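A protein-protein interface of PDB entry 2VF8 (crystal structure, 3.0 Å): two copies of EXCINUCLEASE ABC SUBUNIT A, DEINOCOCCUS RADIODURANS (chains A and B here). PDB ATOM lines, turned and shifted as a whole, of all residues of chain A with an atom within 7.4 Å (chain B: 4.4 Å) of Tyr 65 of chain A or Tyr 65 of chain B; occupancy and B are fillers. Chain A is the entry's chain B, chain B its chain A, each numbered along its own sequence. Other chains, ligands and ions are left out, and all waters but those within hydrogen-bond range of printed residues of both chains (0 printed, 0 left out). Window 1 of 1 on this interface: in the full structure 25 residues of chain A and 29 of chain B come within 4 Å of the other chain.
OG of Ser 68 of chain B sits at hydrogen-bond distance from O of Arg 64 of chain B (3.4 Å).
The side-chain carboxylate of Glu 60 of chain A lies within salt-bridge range of the guanidinium group of Arg 64 of chain A, 3.0 Å away.
The backbone carbonyl oxygen (O) of Arg 64 of chain A lies within hydrogen-bond range of the side-chain hydroxyl (OG) of Ser 68 of chain A (3.3 Å).
O of Pro 93 of chain A lies within hydrogen-bond range of N of Val 402 of chain A (2.9 Å).
Among the printed residues, pairs that only touch across the chains: Leu 398 of chain A with Ser 68 of chain B (3.1 Å), Tyr 65 of chain A with Tyr 65 of chain B (3.4 Å), Phe 399 of chain A with Pro 93 of chain B (3.4 Å), Ser 68 of chain A with Val 95 of chain B (3.4 Å), Arg 64 of chain A with Leu 398 of chain B (3.5 Å), Pro 93 of chain A with Pro 93 of chain B (3.5 Å), Tyr 65 of chain A with Leu 398 of chain B (3.6 Å), Gly 400 of chain A with Pro 93 of chain B (3.6 Å), Val 69 of chain A with Val 95 of chain B (3.7 Å), Ser 396 of chain A with Ser 68 of chain B (3.7 Å), Tyr 65 of chain A with Val 95 of chain B (3.7 Å), Ser 68 of chain A with Leu 398 of chain B (3.7 Å), Leu 398 of chain A with Arg 64 of chain B (3.9 Å), Val 69 of chain A with Ala 94 of chain B (3.9 Å) and Tyr 65 of chain A with Pro 93 of chain B (3.99 Å).
Of the printed residues of chain B, Tyr 65 of chain A touches Tyr 65, Pro 93, Ala 94, Val 95 and Leu 398.
Printed residues of chain A within 4 Å of Tyr 65 of chain B: Tyr 65 (3.4 Å) and Ala 94 (3.1 Å).
Of the printed residues of chain B, Gly 400 of chain A touches Pro 93 (3.6 Å).
Of the printed residues of chain A, Arg 64 of chain B touches Leu 398.
Of the printed residues of chain B, Val 69 of chain A touches Ala 94 (3.9 Å) and Val 95 (3.7 Å).
Of the printed residues of chain A, Ala 94 of chain B touches Tyr 65 (3.0 Å) and Val 69 (3.9 Å).
Gln 62 of chain A touches none of the printed residues of chain B.
Arg 64 of chain A touches Leu 398 of chain B, and with the chains exchanged Leu 398 of chain A touches Arg 64 of chain B.
Tyr 65 of chain A touches Leu 398 of chain B, but with the chains exchanged Leu 398 of chain A does not touch Tyr 65 of chain B (4.2 Å).
Ser 68 of chain A touches Val 95 of chain B, but with the chains exchanged Val 95 of chain A does not touch Ser 68 of chain B (4.1 Å).
Val 69 of chain A touches Ala 94 of chain B, but with the chains exchanged Ala 94 of chain A does not touch Val 69 of chain B (4.4 Å).
13 positions are printed for both chains.
Of the 17 pairs that touch across the chains among the printed residues, 8 have their exchanged pair printed and touching as well.
OH of Tyr 65 of chain B sits at hydrogen-bond distance from O of Ala 94 of chain A.
OH of Tyr 65 of chain A is in hydrogen-bond range of O of Ala 94 of chain B (3.0 Å).
Printed residues of chain B that touch a printed residue of chain A: Arg 64, Tyr 65, Ser 68, Pro 93, Ala 94, Val 95 and Leu 398.
Hydrophobic or aromatic side chains of chain B within 4 Å of the printed part of chain A: Tyr 65, Pro 93, Val 95 and Leu 398.
Hydrophobic or aromatic side chains of chain A within 4 Å of the printed part of chain B: Tyr 65, Val 69, Pro 93 and Leu 398.
Among the printed residues, 17 pairs touch across the chains.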
ATOM      1  N   TYR A  58      -5.940  18.843  10.990  1.00  0.00           N
ATOM      2  CA  TYR A  58      -6.448  18.116  12.171  1.00  0.00           C
ATOM      3  C   TYR A  58      -6.601  16.565  11.904  1.00  0.00           C
ATOM      4  O   TYR A  58      -6.009  15.643  12.598  1.00  0.00           O
ATOM      5  CB  TYR A  58      -7.826  18.769  12.756  1.00  0.00           C
ATOM      6  CG  TYR A  58      -8.441  17.895  13.778  1.00  0.00           C
ATOM      7  CD1 TYR A  58      -7.813  17.742  15.006  1.00  0.00           C
ATOM      8  CD2 TYR A  58      -9.592  17.121  13.548  1.00  0.00           C
ATOM      9  CE1 TYR A  58      -8.375  16.887  16.021  1.00  0.00           C
ATOM     10  CE2 TYR A  58     -10.138  16.251  14.492  1.00  0.00           C
ATOM     11  CZ  TYR A  58      -9.535  16.134  15.752  1.00  0.00           C
ATOM     12  OH  TYR A  58     -10.059  15.325  16.741  1.00  0.00           O
ATOM     13  N   ALA A  59      -7.658  16.182  11.131  1.00  0.00           N
ATOM     14  CA  ALA A  59      -7.989  14.779  10.756  1.00  0.00           C
ATOM     15  C   ALA A  59      -6.819  13.827  10.571  1.00  0.00           C
ATOM     16  O   ALA A  59      -6.882  12.704  11.041  1.00  0.00           O
ATOM     17  CB  ALA A  59      -8.768  14.776   9.508  1.00  0.00           C
ATOM     18  N   GLU A  60      -5.780  14.259   9.844  1.00  0.00           N
ATOM     19  CA  GLU A  60      -4.538  13.518   9.730  1.00  0.00           C
ATOM     20  C   GLU A  60      -3.716  13.521  11.045  1.00  0.00           C
ATOM     21  O   GLU A  60      -3.034  12.571  11.331  1.00  0.00           O
ATOM     22  CB  GLU A  60      -3.730  14.063   8.545  1.00  0.00           C
ATOM     23  CG  GLU A  60      -2.439  13.297   8.232  1.00  0.00           C
ATOM     24  CD  GLU A  60      -2.627  11.995   7.422  1.00  0.00           C
ATOM     25  OE1 GLU A  60      -3.749  11.708   6.925  1.00  0.00           O
ATOM     26  OE2 GLU A  60      -1.613  11.258   7.274  1.00  0.00           O
ATOM     27  N   ALA A  61      -3.763  14.556  11.867  1.00  0.00           N
ATOM     28  CA  ALA A  61      -2.951  14.496  13.102  1.00  0.00           C
ATOM     29  C   ALA A  61      -3.417  13.356  14.049  1.00  0.00           C
ATOM     30  O   ALA A  61      -2.590  12.638  14.618  1.00  0.00           O
ATOM     31  CB  ALA A  61      -2.852  15.856  13.808  1.00  0.00           C
ATOM     32  N   GLN A  62      -4.725  13.175  14.185  1.00  0.00           N
ATOM     33  CA  GLN A  62      -5.273  11.962  14.756  1.00  0.00           C
ATOM     34  C   GLN A  62      -5.020  10.650  14.008  1.00  0.00           C
ATOM     35  O   GLN A  62      -4.582   9.655  14.629  1.00  0.00           O
ATOM     36  CB  GLN A  62      -6.743  12.088  14.841  1.00  0.00           C
ATOM     37  CG  GLN A  62      -7.098  13.245  15.627  1.00  0.00           C
ATOM     38  CD  GLN A  62      -8.310  12.978  16.436  1.00  0.00           C
ATOM     39  OE1 GLN A  62      -8.273  13.165  17.649  1.00  0.00           O
ATOM     40  NE2 GLN A  62      -9.406  12.526  15.783  1.00  0.00           N
ATOM     41  N   ARG A  63      -5.325  10.584  12.710  1.00  0.00           N
ATOM     42  CA  ARG A  63      -5.064   9.322  12.014  1.00  0.00           C
ATOM     43  C   ARG A  63      -3.689   8.830  12.390  1.00  0.00           C
ATOM     44  O   ARG A  63      -3.526   7.684  12.757  1.00  0.00           O
ATOM     45  CB  ARG A  63      -5.134   9.431  10.512  1.00  0.00           C
ATOM     46  CG  ARG A  63      -5.835   8.244   9.915  1.00  0.00           C
ATOM     47  CD  ARG A  63      -5.339   8.019   8.532  1.00  0.00           C
ATOM     48  NE  ARG A  63      -4.200   7.098   8.568  1.00  0.00           N
ATOM     49  CZ  ARG A  63      -2.942   7.451   8.340  1.00  0.00           C
ATOM     50  NH1 ARG A  63      -2.635   8.716   8.038  1.00  0.00           N
ATOM     51  NH2 ARG A  63      -1.997   6.529   8.402  1.00  0.00           N
ATOM     52  N   ARG A  64      -2.705   9.706  12.370  1.00  0.00           N
ATOM     53  CA  ARG A  64      -1.401   9.294  12.796  1.00  0.00           C
ATOM     54  C   ARG A  64      -1.324   8.965  14.272  1.00  0.00           C
ATOM     55  O   ARG A  64      -0.735   7.952  14.658  1.00  0.00           O
ATOM     56  CB  ARG A  64      -0.344  10.335  12.472  1.00  0.00           C
ATOM     57  CG  ARG A  64       0.230  10.219  11.116  1.00  0.00           C
ATOM     58  CD  ARG A  64      -0.351  11.295  10.352  1.00  0.00           C
ATOM     59  NE  ARG A  64       0.500  11.786   9.291  1.00  0.00           N
ATOM     60  CZ  ARG A  64       1.353  12.785   9.445  1.00  0.00           C
ATOM     61  NH1 ARG A  64       1.487  13.371  10.649  1.00  0.00           N
ATOM     62  NH2 ARG A  64       2.043  13.200   8.393  1.00  0.00           N
ATOM     63  N   TYR A  65      -1.887   9.816  15.108  1.00  0.00           N
ATOM     64  CA  TYR A  65      -1.517   9.725  16.512  1.00  0.00           C
ATOM     65  C   TYR A  65      -2.177   8.570  17.189  1.00  0.00           C
ATOM     66  O   TYR A  65      -1.562   7.951  18.032  1.00  0.00           O
ATOM     67  CB  TYR A  65      -1.726  11.024  17.298  1.00  0.00           C
ATOM     68  CG  TYR A  65      -1.357  10.887  18.762  1.00  0.00           C
ATOM     69  CD1 TYR A  65      -0.065  11.087  19.209  1.00  0.00           C
ATOM     70  CD2 TYR A  65      -2.326  10.554  19.697  1.00  0.00           C
ATOM     71  CE1 TYR A  65       0.237  10.963  20.557  1.00  0.00           C
ATOM     72  CE2 TYR A  65      -2.032  10.421  21.029  1.00  0.00           C
ATOM     73  CZ  TYR A  65      -0.763  10.614  21.459  1.00  0.00           C
ATOM     74  OH  TYR A  65      -0.538  10.439  22.811  1.00  0.00           O
ATOM     75  N   LEU A  66      -3.406   8.255  16.816  1.00  0.00           N
ATOM     76  CA  LEU A  66      -4.069   7.109  17.442  1.00  0.00           C
ATOM     77  C   LEU A  66      -3.550   5.793  16.898  1.00  0.00           C
ATOM     78  O   LEU A  66      -3.414   4.824  17.624  1.00  0.00           O
ATOM     79  CB  LEU A  66      -5.585   7.169  17.260  1.00  0.00           C
ATOM     80  CG  LEU A  66      -6.267   8.381  17.865  1.00  0.00           C
ATOM     81  CD1 LEU A  66      -7.700   8.414  17.357  1.00  0.00           C
ATOM     82  CD2 LEU A  66      -6.145   8.366  19.429  1.00  0.00           C
ATOM     83  N   GLU A  67      -3.282   5.764  15.605  1.00  0.00           N
ATOM     84  CA  GLU A  67      -2.800   4.573  15.025  1.00  0.00           C
ATOM     85  C   GLU A  67      -1.493   4.235  15.721  1.00  0.00           C
ATOM     86  O   GLU A  67      -1.243   3.085  16.028  1.00  0.00           O
ATOM     87  CB  GLU A  67      -2.678   4.731  13.518  1.00  0.00           C
ATOM     88  CG  GLU A  67      -3.987   4.418  12.785  1.00  0.00           C
ATOM     89  CD  GLU A  67      -3.891   4.603  11.270  1.00  0.00           C
ATOM     90  OE1 GLU A  67      -2.819   5.011  10.794  1.00  0.00           O
ATOM     91  OE2 GLU A  67      -4.871   4.367  10.531  1.00  0.00           O
ATOM     92  N   SER A  68      -0.684   5.234  16.038  1.00  0.00           N
ATOM     93  CA  SER A  68       0.534   4.969  16.775  1.00  0.00           C
ATOM     94  C   SER A  68       0.324   4.583  18.234  1.00  0.00           C
ATOM     95  O   SER A  68       1.188   3.924  18.813  1.00  0.00           O
ATOM     96  CB  SER A  68       1.477   6.145  16.689  1.00  0.00           C
ATOM     97  OG  SER A  68       1.995   6.236  15.377  1.00  0.00           O
ATOM     98  N   VAL A  69      -0.810   4.973  18.829  1.00  0.00           N
ATOM     99  CA  VAL A  69      -1.074   4.675  20.241  1.00  0.00           C
ATOM    100  C   VAL A  69      -1.925   3.407  20.514  1.00  0.00           C
ATOM    101  O   VAL A  69      -1.921   2.892  21.627  1.00  0.00           O
ATOM    102  CB  VAL A  69      -1.453   5.968  21.044  1.00  0.00           C
ATOM    103  CG1 VAL A  69      -2.263   5.697  22.304  1.00  0.00           C
ATOM    104  CG2 VAL A  69      -0.199   6.702  21.446  1.00  0.00           C
ATOM    105  N   SER A  70      -2.611   2.867  19.506  1.00  0.00           N
ATOM    106  CA  SER A  70      -3.176   1.510  19.625  1.00  0.00           C
ATOM    107  C   SER A  70      -3.074   0.726  18.309  1.00  0.00           C
ATOM    108  O   SER A  70      -4.095   0.314  17.731  1.00  0.00           O
ATOM    109  CB  SER A  70      -4.605   1.552  20.147  1.00  0.00           C
ATOM    110  OG  SER A  70      -5.421   2.259  19.243  1.00  0.00           O
ATOM    111  N   ARG A  74      -7.137   1.122  16.388  1.00  0.00           N
ATOM    112  CA  ARG A  74      -7.524   2.198  15.498  1.00  0.00           C
ATOM    113  C   ARG A  74      -7.400   1.791  14.052  1.00  0.00           C
ATOM    114  O   ARG A  74      -8.331   1.977  13.288  1.00  0.00           O
ATOM    115  CB  ARG A  74      -6.647   3.422  15.734  1.00  0.00           C
ATOM    116  CG  ARG A  74      -7.198   4.748  15.144  1.00  0.00           C
ATOM    117  CD  ARG A  74      -7.570   4.692  13.635  1.00  0.00           C
ATOM    118  NE  ARG A  74      -8.036   5.986  13.122  1.00  0.00           N
ATOM    119  CZ  ARG A  74      -8.605   6.174  11.935  1.00  0.00           C
ATOM    120  NH1 ARG A  74      -8.820   5.164  11.102  1.00  0.00           N
ATOM    121  NH2 ARG A  74      -8.964   7.392  11.587  1.00  0.00           N
ATOM    122  N   PRO A  92       2.351  18.606  14.358  1.00  0.00           N
ATOM    123  CA  PRO A  92       2.295  18.050  15.730  1.00  0.00           C
ATOM    124  C   PRO A  92       0.923  17.461  15.938  1.00  0.00           C
ATOM    125  O   PRO A  92       0.097  17.580  15.048  1.00  0.00           O
ATOM    126  CB  PRO A  92       2.526  19.274  16.647  1.00  0.00           C
ATOM    127  CG  PRO A  92       2.985  20.355  15.739  1.00  0.00           C
ATOM    128  CD  PRO A  92       2.329  20.068  14.390  1.00  0.00           C
ATOM    129  N   PRO A  93       0.676  16.862  17.108  1.00  0.00           N
ATOM    130  CA  PRO A  93      -0.611  16.207  17.299  1.00  0.00           C
ATOM    131  C   PRO A  93      -1.639  17.295  17.641  1.00  0.00           C
ATOM    132  O   PRO A  93      -1.232  18.406  18.094  1.00  0.00           O
ATOM    133  CB  PRO A  93      -0.349  15.258  18.479  1.00  0.00           C
ATOM    134  CG  PRO A  93       1.151  15.443  18.866  1.00  0.00           C
ATOM    135  CD  PRO A  93       1.511  16.797  18.324  1.00  0.00           C
ATOM    136  N   ALA A  94      -2.930  16.996  17.431  1.00  0.00           N
ATOM    137  CA  ALA A  94      -3.936  18.040  17.445  1.00  0.00           C
ATOM    138  C   ALA A  94      -5.045  17.836  18.432  1.00  0.00           C
ATOM    139  O   ALA A  94      -5.331  16.718  18.779  1.00  0.00           O
ATOM    140  CB  ALA A  94      -4.503  18.200  16.063  1.00  0.00           C
ATOM    141  N   VAL A  95      -5.682  18.930  18.843  1.00  0.00           N
ATOM    142  CA  VAL A  95      -6.937  18.911  19.584  1.00  0.00           C
ATOM    143  C   VAL A  95      -7.909  19.874  18.959  1.00  0.00           C
ATOM    144  O   VAL A  95      -7.599  21.087  18.804  1.00  0.00           O
ATOM    145  CB  VAL A  95      -6.746  19.298  21.018  1.00  0.00           C
ATOM    146  CG1 VAL A  95      -8.070  19.383  21.694  1.00  0.00           C
ATOM    147  CG2 VAL A  95      -5.821  18.279  21.707  1.00  0.00           C
ATOM    148  N   ALA A  96      -9.073  19.306  18.591  1.00  0.00           N
ATOM    149  CA  ALA A  96     -10.179  20.031  17.996  1.00  0.00           C
ATOM    150  C   ALA A  96     -11.122  20.468  19.085  1.00  0.00           C
ATOM    151  O   ALA A  96     -11.295  19.773  20.081  1.00  0.00           O
ATOM    152  CB  ALA A  96     -10.877  19.135  17.055  1.00  0.00           C
ATOM    153  N   SER A 396      -5.822  23.518  31.524  1.00  0.00           N
ATOM    154  CA  SER A 396      -5.661  22.071  31.245  1.00  0.00           C
ATOM    155  C   SER A 396      -4.239  21.550  30.861  1.00  0.00           C
ATOM    156  O   SER A 396      -4.062  20.347  30.700  1.00  0.00           O
ATOM    157  CB  SER A 396      -6.711  21.557  30.242  1.00  0.00           C
ATOM    158  OG  SER A 396      -6.094  21.126  28.992  1.00  0.00           O
ATOM    159  N   LEU A 398      -1.737  21.237  28.434  1.00  0.00           N
ATOM    160  CA  LEU A 398      -1.197  20.576  27.284  1.00  0.00           C
ATOM    161  C   LEU A 398      -0.080  21.385  26.697  1.00  0.00           C
ATOM    162  O   LEU A 398      -0.103  22.617  26.769  1.00  0.00           O
ATOM    163  CB  LEU A 398      -2.298  20.475  26.263  1.00  0.00           C
ATOM    164  CG  LEU A 398      -2.944  19.116  26.320  1.00  0.00           C
ATOM    165  CD1 LEU A 398      -4.305  19.255  25.727  1.00  0.00           C
ATOM    166  CD2 LEU A 398      -2.074  18.256  25.452  1.00  0.00           C
ATOM    167  N   PHE A 399       0.895  20.722  26.083  1.00  0.00           N
ATOM    168  CA  PHE A 399       2.011  21.463  25.524  1.00  0.00           C
ATOM    169  C   PHE A 399       2.454  20.768  24.288  1.00  0.00           C
ATOM    170  O   PHE A 399       2.415  19.552  24.240  1.00  0.00           O
ATOM    171  CB  PHE A 399       3.152  21.536  26.537  1.00  0.00           C
ATOM    172  CG  PHE A 399       4.459  21.960  25.958  1.00  0.00           C
ATOM    173  CD1 PHE A 399       4.795  23.299  25.893  1.00  0.00           C
ATOM    174  CD2 PHE A 399       5.346  21.028  25.482  1.00  0.00           C
ATOM    175  CE1 PHE A 399       6.015  23.711  25.389  1.00  0.00           C
ATOM    176  CE2 PHE A 399       6.569  21.420  24.972  1.00  0.00           C
ATOM    177  CZ  PHE A 399       6.915  22.777  24.928  1.00  0.00           C
ATOM    178  N   GLY A 400       2.866  21.548  23.294  1.00  0.00           N
ATOM    179  CA  GLY A 400       3.153  21.054  21.954  1.00  0.00           C
ATOM    180  C   GLY A 400       1.935  20.541  21.204  1.00  0.00           C
ATOM    181  O   GLY A 400       1.983  19.418  20.834  1.00  0.00           O
ATOM    182  N   VAL A 401       0.890  21.341  20.903  1.00  0.00           N
ATOM    183  CA  VAL A 401      -0.267  20.771  20.235  1.00  0.00           C
ATOM    184  C   VAL A 401      -0.859  21.733  19.208  1.00  0.00           C
ATOM    185  O   VAL A 401      -0.497  22.925  19.264  1.00  0.00           O
ATOM    186  CB  VAL A 401      -1.199  20.401  21.327  1.00  0.00           C
ATOM    187  CG1 VAL A 401      -0.429  19.605  22.362  1.00  0.00           C
ATOM    188  CG2 VAL A 401      -1.782  21.689  22.007  1.00  0.00           C
ATOM    189  N   VAL A 402      -1.744  21.263  18.304  1.00  0.00           N
ATOM    190  CA  VAL A 402      -2.434  22.175  17.423  1.00  0.00           C
ATOM    191  C   VAL A 402      -3.852  22.092  17.830  1.00  0.00           C
ATOM    192  O   VAL A 402      -4.506  21.051  17.620  1.00  0.00           O
ATOM    193  CB  VAL A 402      -2.211  21.779  15.964  1.00  0.00           C
ATOM    194  CG1 VAL A 402      -2.570  22.945  15.037  1.00  0.00           C
ATOM    195  CG2 VAL A 402      -0.730  21.450  15.778  1.00  0.00           C
ATOM    196  N   ALA B  61       1.491  12.424  30.534  1.00  0.00           N
ATOM    197  CA  ALA B  61       1.301  12.947  29.204  1.00  0.00           C
ATOM    198  C   ALA B  61       0.215  12.176  28.450  1.00  0.00           C
ATOM    199  O   ALA B  61      -0.575  12.784  27.755  1.00  0.00           O
ATOM    200  CB  ALA B  61       2.644  13.015  28.433  1.00  0.00           C
ATOM    201  N   GLN B  62       0.157  10.859  28.600  1.00  0.00           N
ATOM    202  CA  GLN B  62      -0.998  10.065  28.167  1.00  0.00           C
ATOM    203  C   GLN B  62      -2.299  10.719  28.491  1.00  0.00           C
ATOM    204  O   GLN B  62      -3.164  10.852  27.647  1.00  0.00           O
ATOM    205  CB  GLN B  62      -1.061   8.766  28.956  1.00  0.00           C
ATOM    206  CG  GLN B  62      -0.787   7.541  28.187  1.00  0.00           C
ATOM    207  CD  GLN B  62      -1.654   7.451  27.000  1.00  0.00           C
ATOM    208  OE1 GLN B  62      -1.519   8.249  26.036  1.00  0.00           O
ATOM    209  NE2 GLN B  62      -2.595   6.483  27.041  1.00  0.00           N
ATOM    210  N   ARG B  63      -2.430  11.089  29.758  1.00  0.00           N
ATOM    211  CA  ARG B  63      -3.681  11.483  30.363  1.00  0.00           C
ATOM    212  C   ARG B  63      -4.124  12.892  30.033  1.00  0.00           C
ATOM    213  O   ARG B  63      -5.302  13.117  29.868  1.00  0.00           O
ATOM    214  CB  ARG B  63      -3.565  11.352  31.866  1.00  0.00           C
ATOM    215  CG  ARG B  63      -4.874  11.322  32.569  1.00  0.00           C
ATOM    216  CD  ARG B  63      -4.667  11.455  34.069  1.00  0.00           C
ATOM    217  NE  ARG B  63      -4.857  12.846  34.478  1.00  0.00           N
ATOM    218  CZ  ARG B  63      -3.903  13.773  34.500  1.00  0.00           C
ATOM    219  NH1 ARG B  63      -2.656  13.465  34.156  1.00  0.00           N
ATOM    220  NH2 ARG B  63      -4.211  15.010  34.879  1.00  0.00           N
ATOM    221  N   ARG B  64      -3.217  13.856  29.952  1.00  0.00           N
ATOM    222  CA  ARG B  64      -3.655  15.219  29.751  1.00  0.00           C
ATOM    223  C   ARG B  64      -4.176  15.316  28.361  1.00  0.00           C
ATOM    224  O   ARG B  64      -4.963  16.214  28.030  1.00  0.00           O
ATOM    225  CB  ARG B  64      -2.513  16.191  29.865  1.00  0.00           C
ATOM    226  CG  ARG B  64      -1.901  16.243  31.186  1.00  0.00           C
ATOM    227  CD  ARG B  64      -0.580  16.841  31.035  1.00  0.00           C
ATOM    228  NE  ARG B  64      -0.162  17.345  32.315  1.00  0.00           N
ATOM    229  CZ  ARG B  64       0.968  18.001  32.490  1.00  0.00           C
ATOM    230  NH1 ARG B  64       1.780  18.189  31.439  1.00  0.00           N
ATOM    231  NH2 ARG B  64       1.280  18.457  33.704  1.00  0.00           N
ATOM    232  N   TYR B  65      -3.713  14.385  27.540  1.00  0.00           N
ATOM    233  CA  TYR B  65      -4.095  14.356  26.159  1.00  0.00           C
ATOM    234  C   TYR B  65      -5.420  13.671  26.008  1.00  0.00           C
ATOM    235  O   TYR B  65      -6.287  14.173  25.332  1.00  0.00           O
ATOM    236  CB  TYR B  65      -3.042  13.641  25.334  1.00  0.00           C
ATOM    237  CG  TYR B  65      -3.341  13.714  23.872  1.00  0.00           C
ATOM    238  CD1 TYR B  65      -2.965  14.826  23.133  1.00  0.00           C
ATOM    239  CD2 TYR B  65      -4.024  12.686  23.223  1.00  0.00           C
ATOM    240  CE1 TYR B  65      -3.250  14.917  21.773  1.00  0.00           C
ATOM    241  CE2 TYR B  65      -4.312  12.772  21.855  1.00  0.00           C
ATOM    242  CZ  TYR B  65      -3.919  13.895  21.137  1.00  0.00           C
ATOM    243  OH  TYR B  65      -4.191  14.012  19.788  1.00  0.00           O
ATOM    244  N   LEU B  66      -5.577  12.524  26.646  1.00  0.00           N
ATOM    245  CA  LEU B  66      -6.802  11.758  26.486  1.00  0.00           C
ATOM    246  C   LEU B  66      -8.011  12.515  26.969  1.00  0.00           C
ATOM    247  O   LEU B  66      -9.085  12.416  26.376  1.00  0.00           O
ATOM    248  CB  LEU B  66      -6.708  10.402  27.159  1.00  0.00           C
ATOM    249  CG  LEU B  66      -5.953   9.454  26.219  1.00  0.00           C
ATOM    250  CD1 LEU B  66      -5.379   8.256  26.978  1.00  0.00           C
ATOM    251  CD2 LEU B  66      -6.792   8.991  25.006  1.00  0.00           C
ATOM    252  N   GLU B  67      -7.827  13.309  28.015  1.00  0.00           N
ATOM    253  CA  GLU B  67      -8.894  14.132  28.559  1.00  0.00           C
ATOM    254  C   GLU B  67      -9.299  15.318  27.705  1.00  0.00           C
ATOM    255  O   GLU B  67     -10.365  15.877  27.892  1.00  0.00           O
ATOM    256  CB  GLU B  67      -8.457  14.632  29.904  1.00  0.00           C
ATOM    257  CG  GLU B  67      -8.252  13.508  30.867  1.00  0.00           C
ATOM    258  CD  GLU B  67      -7.635  13.977  32.145  1.00  0.00           C
ATOM    259  OE1 GLU B  67      -7.188  15.147  32.189  1.00  0.00           O
ATOM    260  OE2 GLU B  67      -7.590  13.179  33.105  1.00  0.00           O
ATOM    261  N   SER B  68      -8.429  15.721  26.790  1.00  0.00           N
ATOM    262  CA  SER B  68      -8.727  16.823  25.890  1.00  0.00           C
ATOM    263  C   SER B  68      -9.362  16.334  24.615  1.00  0.00           C
ATOM    264  O   SER B  68     -10.301  16.946  24.106  1.00  0.00           O
ATOM    265  CB  SER B  68      -7.469  17.610  25.580  1.00  0.00           C
ATOM    266  OG  SER B  68      -7.147  18.420  26.696  1.00  0.00           O
ATOM    267  N   VAL B  69      -8.845  15.231  24.107  1.00  0.00           N
ATOM    268  CA  VAL B  69      -9.422  14.581  22.957  1.00  0.00           C
ATOM    269  C   VAL B  69     -10.813  13.993  23.223  1.00  0.00           C
ATOM    270  O   VAL B  69     -11.734  14.243  22.463  1.00  0.00           O
ATOM    271  CB  VAL B  69      -8.486  13.506  22.451  1.00  0.00           C
ATOM    272  CG1 VAL B  69      -9.232  12.523  21.541  1.00  0.00           C
ATOM    273  CG2 VAL B  69      -7.338  14.158  21.737  1.00  0.00           C
ATOM    274  N   PRO B  93       2.897  15.401  23.788  1.00  0.00           N
ATOM    275  CA  PRO B  93       2.162  14.122  23.703  1.00  0.00           C
ATOM    276  C   PRO B  93       3.060  12.841  23.575  1.00  0.00           C
ATOM    277  O   PRO B  93       4.038  12.858  22.820  1.00  0.00           O
ATOM    278  CB  PRO B  93       1.320  14.313  22.442  1.00  0.00           C
ATOM    279  CG  PRO B  93       1.104  15.821  22.394  1.00  0.00           C
ATOM    280  CD  PRO B  93       2.383  16.410  22.853  1.00  0.00           C
ATOM    281  N   ALA B  94       2.772  11.749  24.290  1.00  0.00           N
ATOM    282  CA  ALA B  94       3.716  10.633  24.258  1.00  0.00           C
ATOM    283  C   ALA B  94       3.216   9.387  23.569  1.00  0.00           C
ATOM    284  O   ALA B  94       2.017   9.114  23.542  1.00  0.00           O
ATOM    285  CB  ALA B  94       4.183  10.313  25.621  1.00  0.00           C
ATOM    286  N   VAL B  95       4.145   8.638  22.987  1.00  0.00           N
ATOM    287  CA  VAL B  95       3.840   7.351  22.412  1.00  0.00           C
ATOM    288  C   VAL B  95       4.738   6.263  22.987  1.00  0.00           C
ATOM    289  O   VAL B  95       5.971   6.329  22.902  1.00  0.00           O
ATOM    290  CB  VAL B  95       3.862   7.366  20.883  1.00  0.00           C
ATOM    291  CG1 VAL B  95       3.459   6.024  20.329  1.00  0.00           C
ATOM    292  CG2 VAL B  95       2.873   8.368  20.374  1.00  0.00           C
ATOM    293  N   LEU B 398       4.614  10.547  12.586  1.00  0.00           N
ATOM    294  CA  LEU B 398       4.442  11.504  13.724  1.00  0.00           C
ATOM    295  C   LEU B 398       5.565  12.520  13.851  1.00  0.00           C
ATOM    296  O   LEU B 398       6.731  12.215  13.603  1.00  0.00           O
ATOM    297  CB  LEU B 398       4.335  10.825  15.101  1.00  0.00           C
ATOM    298  CG  LEU B 398       3.337   9.722  15.424  1.00  0.00           C
ATOM    299  CD1 LEU B 398       3.656   9.306  16.816  1.00  0.00           C
ATOM    300  CD2 LEU B 398       1.878  10.191  15.281  1.00  0.00           C
